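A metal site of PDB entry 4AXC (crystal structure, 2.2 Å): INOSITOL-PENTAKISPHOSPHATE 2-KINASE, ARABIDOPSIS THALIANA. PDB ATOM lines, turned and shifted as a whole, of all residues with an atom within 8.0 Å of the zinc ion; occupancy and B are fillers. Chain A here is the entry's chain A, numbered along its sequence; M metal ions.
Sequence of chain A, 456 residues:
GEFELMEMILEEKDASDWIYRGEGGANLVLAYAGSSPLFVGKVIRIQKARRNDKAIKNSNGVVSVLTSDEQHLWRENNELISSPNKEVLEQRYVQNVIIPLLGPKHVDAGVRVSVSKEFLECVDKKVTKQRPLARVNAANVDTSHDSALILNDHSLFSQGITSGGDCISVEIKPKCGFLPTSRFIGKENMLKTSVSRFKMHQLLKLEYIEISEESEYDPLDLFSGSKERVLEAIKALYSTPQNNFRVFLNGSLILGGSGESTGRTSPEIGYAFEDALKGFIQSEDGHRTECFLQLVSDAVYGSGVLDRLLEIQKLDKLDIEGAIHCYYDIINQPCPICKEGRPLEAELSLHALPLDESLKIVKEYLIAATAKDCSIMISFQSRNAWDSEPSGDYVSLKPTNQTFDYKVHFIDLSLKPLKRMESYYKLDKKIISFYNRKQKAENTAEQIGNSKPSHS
A ring nitrogen (ND1) of His 351 is in hydrogen-bond range of the side-chain carboxylate (OD2) of Asp 329 (2.8 Å).
A ring nitrogen (NE2) of His 325 sits at hydrogen-bond distance from the backbone carbonyl oxygen (O) of Glu 321 (2.9 Å).
The backbone NH (N) of Ile 337 sits close to the side-chain sulfur (SG) of Cys 335.
Of the 18 residues printed, 4 come within 4 Å of the zinc ion.
The zinc ion is bound by a ring nitrogen (NE2) of His 351 (2.1 Å), a ring nitrogen (ND1) of His 325 (2.3 Å), the side-chain sulfur (SG) of Cys 335 (2.4 Å) and the side-chain sulfur (SG) of Cys 338 (2.4 Å).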
ATOM      1  N   GLU A 321      -4.193  -6.720 -32.551  1.00  0.00           N
ATOM      2  CA  GLU A 321      -5.573  -7.171 -32.813  1.00  0.00           C
ATOM      3  C   GLU A 321      -5.880  -8.535 -32.200  1.00  0.00           C
ATOM      4  O   GLU A 321      -7.042  -8.827 -31.886  1.00  0.00           O
ATOM      5  CB  GLU A 321      -5.895  -7.179 -34.303  1.00  0.00           C
ATOM      6  CG  GLU A 321      -6.107  -5.789 -34.887  1.00  0.00           C
ATOM      7  CD  GLU A 321      -6.597  -5.827 -36.328  1.00  0.00           C
ATOM      8  OE1 GLU A 321      -7.796  -6.062 -36.552  1.00  0.00           O
ATOM      9  OE2 GLU A 321      -5.782  -5.610 -37.230  1.00  0.00           O
ATOM     10  N   GLY A 322      -4.856  -9.357 -31.999  1.00  0.00           N
ATOM     11  CA  GLY A 322      -5.024 -10.576 -31.204  1.00  0.00           C
ATOM     12  C   GLY A 322      -4.832 -10.326 -29.720  1.00  0.00           C
ATOM     13  O   GLY A 322      -5.684 -10.665 -28.892  1.00  0.00           O
ATOM     14  N   ILE A 324      -4.942  -7.752 -27.758  1.00  0.00           N
ATOM     15  CA  ILE A 324      -5.935  -6.893 -27.089  1.00  0.00           C
ATOM     16  C   ILE A 324      -7.053  -7.674 -26.383  1.00  0.00           C
ATOM     17  O   ILE A 324      -7.584  -7.230 -25.366  1.00  0.00           O
ATOM     18  CB  ILE A 324      -6.567  -5.842 -28.054  1.00  0.00           C
ATOM     19  CG1 ILE A 324      -7.499  -4.859 -27.318  1.00  0.00           C
ATOM     20  CG2 ILE A 324      -7.350  -6.523 -29.182  1.00  0.00           C
ATOM     21  CD1 ILE A 324      -6.843  -4.046 -26.223  1.00  0.00           C
ATOM     22  N   HIS A 325      -7.396  -8.848 -26.936  1.00  0.00           N
ATOM     23  CA  HIS A 325      -8.462  -9.681 -26.350  1.00  0.00           C
ATOM     24  C   HIS A 325      -7.989 -10.281 -25.055  1.00  0.00           C
ATOM     25  O   HIS A 325      -8.710 -10.270 -24.057  1.00  0.00           O
ATOM     26  CB  HIS A 325      -8.910 -10.764 -27.315  1.00  0.00           C
ATOM     27  CG  HIS A 325      -9.378 -10.244 -28.661  1.00  0.00           C
ATOM     28  ND1 HIS A 325     -10.657  -9.939 -28.917  1.00  0.00           N
ATOM     29  CD2 HIS A 325      -8.680  -9.990 -29.845  1.00  0.00           C
ATOM     30  CE1 HIS A 325     -10.777  -9.511 -30.190  1.00  0.00           C
ATOM     31  NE2 HIS A 325      -9.564  -9.535 -30.750  1.00  0.00           N
ATOM     32  N   CYS A 326      -6.770 -10.811 -25.054  1.00  0.00           N
ATOM     33  CA  CYS A 326      -6.135 -11.331 -23.848  1.00  0.00           C
ATOM     34  C   CYS A 326      -6.061 -10.269 -22.738  1.00  0.00           C
ATOM     35  O   CYS A 326      -6.188 -10.594 -21.558  1.00  0.00           O
ATOM     36  CB  CYS A 326      -4.725 -11.838 -24.154  1.00  0.00           C
ATOM     37  SG  CYS A 326      -4.630 -13.166 -25.384  1.00  0.00           S
ATOM     38  N   TYR A 327      -5.837  -9.014 -23.137  1.00  0.00           N
ATOM     39  CA  TYR A 327      -5.737  -7.884 -22.195  1.00  0.00           C
ATOM     40  C   TYR A 327      -7.014  -7.761 -21.359  1.00  0.00           C
ATOM     41  O   TYR A 327      -6.955  -7.688 -20.116  1.00  0.00           O
ATOM     42  CB  TYR A 327      -5.444  -6.573 -22.936  1.00  0.00           C
ATOM     43  CG  TYR A 327      -5.658  -5.338 -22.101  1.00  0.00           C
ATOM     44  CD1 TYR A 327      -4.708  -4.936 -21.159  1.00  0.00           C
ATOM     45  CD2 TYR A 327      -6.825  -4.583 -22.228  1.00  0.00           C
ATOM     46  CE1 TYR A 327      -4.917  -3.802 -20.379  1.00  0.00           C
ATOM     47  CE2 TYR A 327      -7.036  -3.458 -21.472  1.00  0.00           C
ATOM     48  CZ  TYR A 327      -6.084  -3.075 -20.544  1.00  0.00           C
ATOM     49  OH  TYR A 327      -6.299  -1.941 -19.786  1.00  0.00           O
ATOM     50  N   TYR A 328      -8.161  -7.742 -22.043  1.00  0.00           N
ATOM     51  CA  TYR A 328      -9.443  -7.602 -21.379  1.00  0.00           C
ATOM     52  C   TYR A 328      -9.793  -8.778 -20.476  1.00  0.00           C
ATOM     53  O   TYR A 328     -10.659  -8.672 -19.605  1.00  0.00           O
ATOM     54  CB  TYR A 328     -10.535  -7.294 -22.402  1.00  0.00           C
ATOM     55  CG  TYR A 328     -10.465  -5.853 -22.885  1.00  0.00           C
ATOM     56  CD1 TYR A 328     -10.780  -4.793 -22.020  1.00  0.00           C
ATOM     57  CD2 TYR A 328     -10.062  -5.553 -24.179  1.00  0.00           C
ATOM     58  CE1 TYR A 328     -10.706  -3.475 -22.449  1.00  0.00           C
ATOM     59  CE2 TYR A 328      -9.983  -4.243 -24.610  1.00  0.00           C
ATOM     60  CZ  TYR A 328     -10.306  -3.210 -23.752  1.00  0.00           C
ATOM     61  OH  TYR A 328     -10.222  -1.906 -24.195  1.00  0.00           O
ATOM     62  N   ASP A 329      -9.093  -9.896 -20.668  1.00  0.00           N
ATOM     63  CA  ASP A 329      -9.240 -11.040 -19.779  1.00  0.00           C
ATOM     64  C   ASP A 329      -8.363 -10.942 -18.535  1.00  0.00           C
ATOM     65  O   ASP A 329      -8.615 -11.623 -17.535  1.00  0.00           O
ATOM     66  CB  ASP A 329      -8.966 -12.340 -20.531  1.00  0.00           C
ATOM     67  CG  ASP A 329     -10.097 -12.728 -21.456  1.00  0.00           C
ATOM     68  OD1 ASP A 329     -11.216 -12.176 -21.286  1.00  0.00           O
ATOM     69  OD2 ASP A 329      -9.870 -13.578 -22.341  1.00  0.00           O
ATOM     70  N   GLN A 333     -12.729  -7.552 -17.654  1.00  0.00           N
ATOM     71  CA  GLN A 333     -13.763  -6.636 -18.133  1.00  0.00           C
ATOM     72  C   GLN A 333     -14.303  -7.195 -19.456  1.00  0.00           C
ATOM     73  O   GLN A 333     -13.550  -7.833 -20.208  1.00  0.00           O
ATOM     74  CB  GLN A 333     -13.171  -5.219 -18.344  1.00  0.00           C
ATOM     75  CG  GLN A 333     -14.189  -4.065 -18.392  1.00  0.00           C
ATOM     76  CD  GLN A 333     -13.603  -2.784 -18.998  1.00  0.00           C
ATOM     77  OE1 GLN A 333     -12.834  -2.045 -18.467  1.00  0.00           O
ATOM     78  NE2 GLN A 333     -13.938  -2.539 -20.273  1.00  0.00           N
ATOM     79  N   PRO A 334     -15.606  -6.991 -19.739  1.00  0.00           N
ATOM     80  CA  PRO A 334     -16.166  -7.355 -21.048  1.00  0.00           C
ATOM     81  C   PRO A 334     -15.367  -6.763 -22.213  1.00  0.00           C
ATOM     82  O   PRO A 334     -14.868  -5.641 -22.101  1.00  0.00           O
ATOM     83  CB  PRO A 334     -17.574  -6.739 -21.004  1.00  0.00           C
ATOM     84  CG  PRO A 334     -17.929  -6.742 -19.562  1.00  0.00           C
ATOM     85  CD  PRO A 334     -16.646  -6.517 -18.806  1.00  0.00           C
ATOM     86  N   CYS A 335     -15.242  -7.504 -23.298  1.00  0.00           N
ATOM     87  CA  CYS A 335     -14.399  -7.094 -24.409  1.00  0.00           C
ATOM     88  C   CYS A 335     -15.106  -6.210 -25.432  1.00  0.00           C
ATOM     89  O   CYS A 335     -15.991  -6.676 -26.157  1.00  0.00           O
ATOM     90  CB  CYS A 335     -13.806  -8.323 -25.113  1.00  0.00           C
ATOM     91  SG  CYS A 335     -12.608  -7.857 -26.363  1.00  0.00           S
ATOM     92  N   PRO A 336     -14.714  -4.924 -25.519  1.00  0.00           N
ATOM     93  CA  PRO A 336     -15.367  -3.979 -26.408  1.00  0.00           C
ATOM     94  C   PRO A 336     -14.973  -4.181 -27.875  1.00  0.00           C
ATOM     95  O   PRO A 336     -15.495  -3.478 -28.759  1.00  0.00           O
ATOM     96  CB  PRO A 336     -14.847  -2.629 -25.920  1.00  0.00           C
ATOM     97  CG  PRO A 336     -13.498  -2.929 -25.366  1.00  0.00           C
ATOM     98  CD  PRO A 336     -13.602  -4.307 -24.768  1.00  0.00           C
ATOM     99  N   ILE A 337     -14.065  -5.119 -28.127  1.00  0.00           N
ATOM    100  CA  ILE A 337     -13.586  -5.398 -29.491  1.00  0.00           C
ATOM    101  C   ILE A 337     -14.488  -6.442 -30.129  1.00  0.00           C
ATOM    102  O   ILE A 337     -14.888  -6.299 -31.290  1.00  0.00           O
ATOM    103  CB  ILE A 337     -12.124  -5.888 -29.499  1.00  0.00           C
ATOM    104  CG1 ILE A 337     -11.213  -5.029 -28.585  1.00  0.00           C
ATOM    105  CG2 ILE A 337     -11.595  -6.013 -30.925  1.00  0.00           C
ATOM    106  CD1 ILE A 337     -11.197  -3.539 -28.876  1.00  0.00           C
ATOM    107  N   CYS A 338     -14.820  -7.478 -29.367  1.00  0.00           N
ATOM    108  CA  CYS A 338     -15.712  -8.550 -29.825  1.00  0.00           C
ATOM    109  C   CYS A 338     -17.154  -8.101 -30.031  1.00  0.00           C
ATOM    110  O   CYS A 338     -17.593  -7.099 -29.460  1.00  0.00           O
ATOM    111  CB  CYS A 338     -15.651  -9.736 -28.854  1.00  0.00           C
ATOM    112  SG  CYS A 338     -14.073 -10.607 -28.891  1.00  0.00           S
ATOM    113  N   GLU A 347     -13.345 -13.231 -32.066  1.00  0.00           N
ATOM    114  CA  GLU A 347     -12.217 -13.990 -31.540  1.00  0.00           C
ATOM    115  C   GLU A 347     -12.576 -14.754 -30.282  1.00  0.00           C
ATOM    116  O   GLU A 347     -12.057 -14.484 -29.196  1.00  0.00           O
ATOM    117  CB  GLU A 347     -11.032 -13.079 -31.279  1.00  0.00           C
ATOM    118  CG  GLU A 347     -10.185 -12.782 -32.511  1.00  0.00           C
ATOM    119  CD  GLU A 347     -10.892 -11.921 -33.539  1.00  0.00           C
ATOM    120  OE1 GLU A 347     -11.867 -11.212 -33.183  1.00  0.00           O
ATOM    121  OE2 GLU A 347     -10.463 -11.952 -34.714  1.00  0.00           O
ATOM    122  N   LEU A 348     -13.452 -15.737 -30.437  1.00  0.00           N
ATOM    123  CA  LEU A 348     -13.942 -16.524 -29.310  1.00  0.00           C
ATOM    124  C   LEU A 348     -12.878 -17.381 -28.629  1.00  0.00           C
ATOM    125  O   LEU A 348     -12.906 -17.558 -27.404  1.00  0.00           O
ATOM    126  CB  LEU A 348     -15.119 -17.397 -29.747  1.00  0.00           C
ATOM    127  CG  LEU A 348     -16.509 -16.772 -29.700  1.00  0.00           C
ATOM    128  CD1 LEU A 348     -17.500 -17.615 -30.494  1.00  0.00           C
ATOM    129  CD2 LEU A 348     -16.991 -16.590 -28.256  1.00  0.00           C
ATOM    130  N   LEU A 350      -9.497 -16.983 -28.238  1.00  0.00           N
ATOM    131  CA  LEU A 350      -8.579 -16.266 -27.347  1.00  0.00           C
ATOM    132  C   LEU A 350      -9.160 -16.049 -25.946  1.00  0.00           C
ATOM    133  O   LEU A 350      -8.414 -16.004 -24.975  1.00  0.00           O
ATOM    134  CB  LEU A 350      -8.164 -14.916 -27.953  1.00  0.00           C
ATOM    135  CG  LEU A 350      -7.342 -14.930 -29.252  1.00  0.00           C
ATOM    136  CD1 LEU A 350      -7.077 -13.506 -29.699  1.00  0.00           C
ATOM    137  CD2 LEU A 350      -6.033 -15.679 -29.058  1.00  0.00           C
ATOM    138  N   HIS A 351     -10.477 -15.935 -25.849  1.00  0.00           N
ATOM    139  CA  HIS A 351     -11.125 -15.794 -24.545  1.00  0.00           C
ATOM    140  C   HIS A 351     -11.328 -17.099 -23.815  1.00  0.00           C
ATOM    141  O   HIS A 351     -11.663 -17.101 -22.628  1.00  0.00           O
ATOM    142  CB  HIS A 351     -12.425 -14.991 -24.694  1.00  0.00           C
ATOM    143  CG  HIS A 351     -12.202 -13.555 -25.081  1.00  0.00           C
ATOM    144  ND1 HIS A 351     -11.699 -12.654 -24.217  1.00  0.00           N
ATOM    145  CD2 HIS A 351     -12.387 -12.885 -26.291  1.00  0.00           C
ATOM    146  CE1 HIS A 351     -11.565 -11.461 -24.846  1.00  0.00           C
ATOM    147  NE2 HIS A 351     -11.981 -11.607 -26.110  1.00  0.00           N
HETATM  148 ZN    ZN M   1     -12.287  -9.995 -27.352  1.00  0.00          ZN
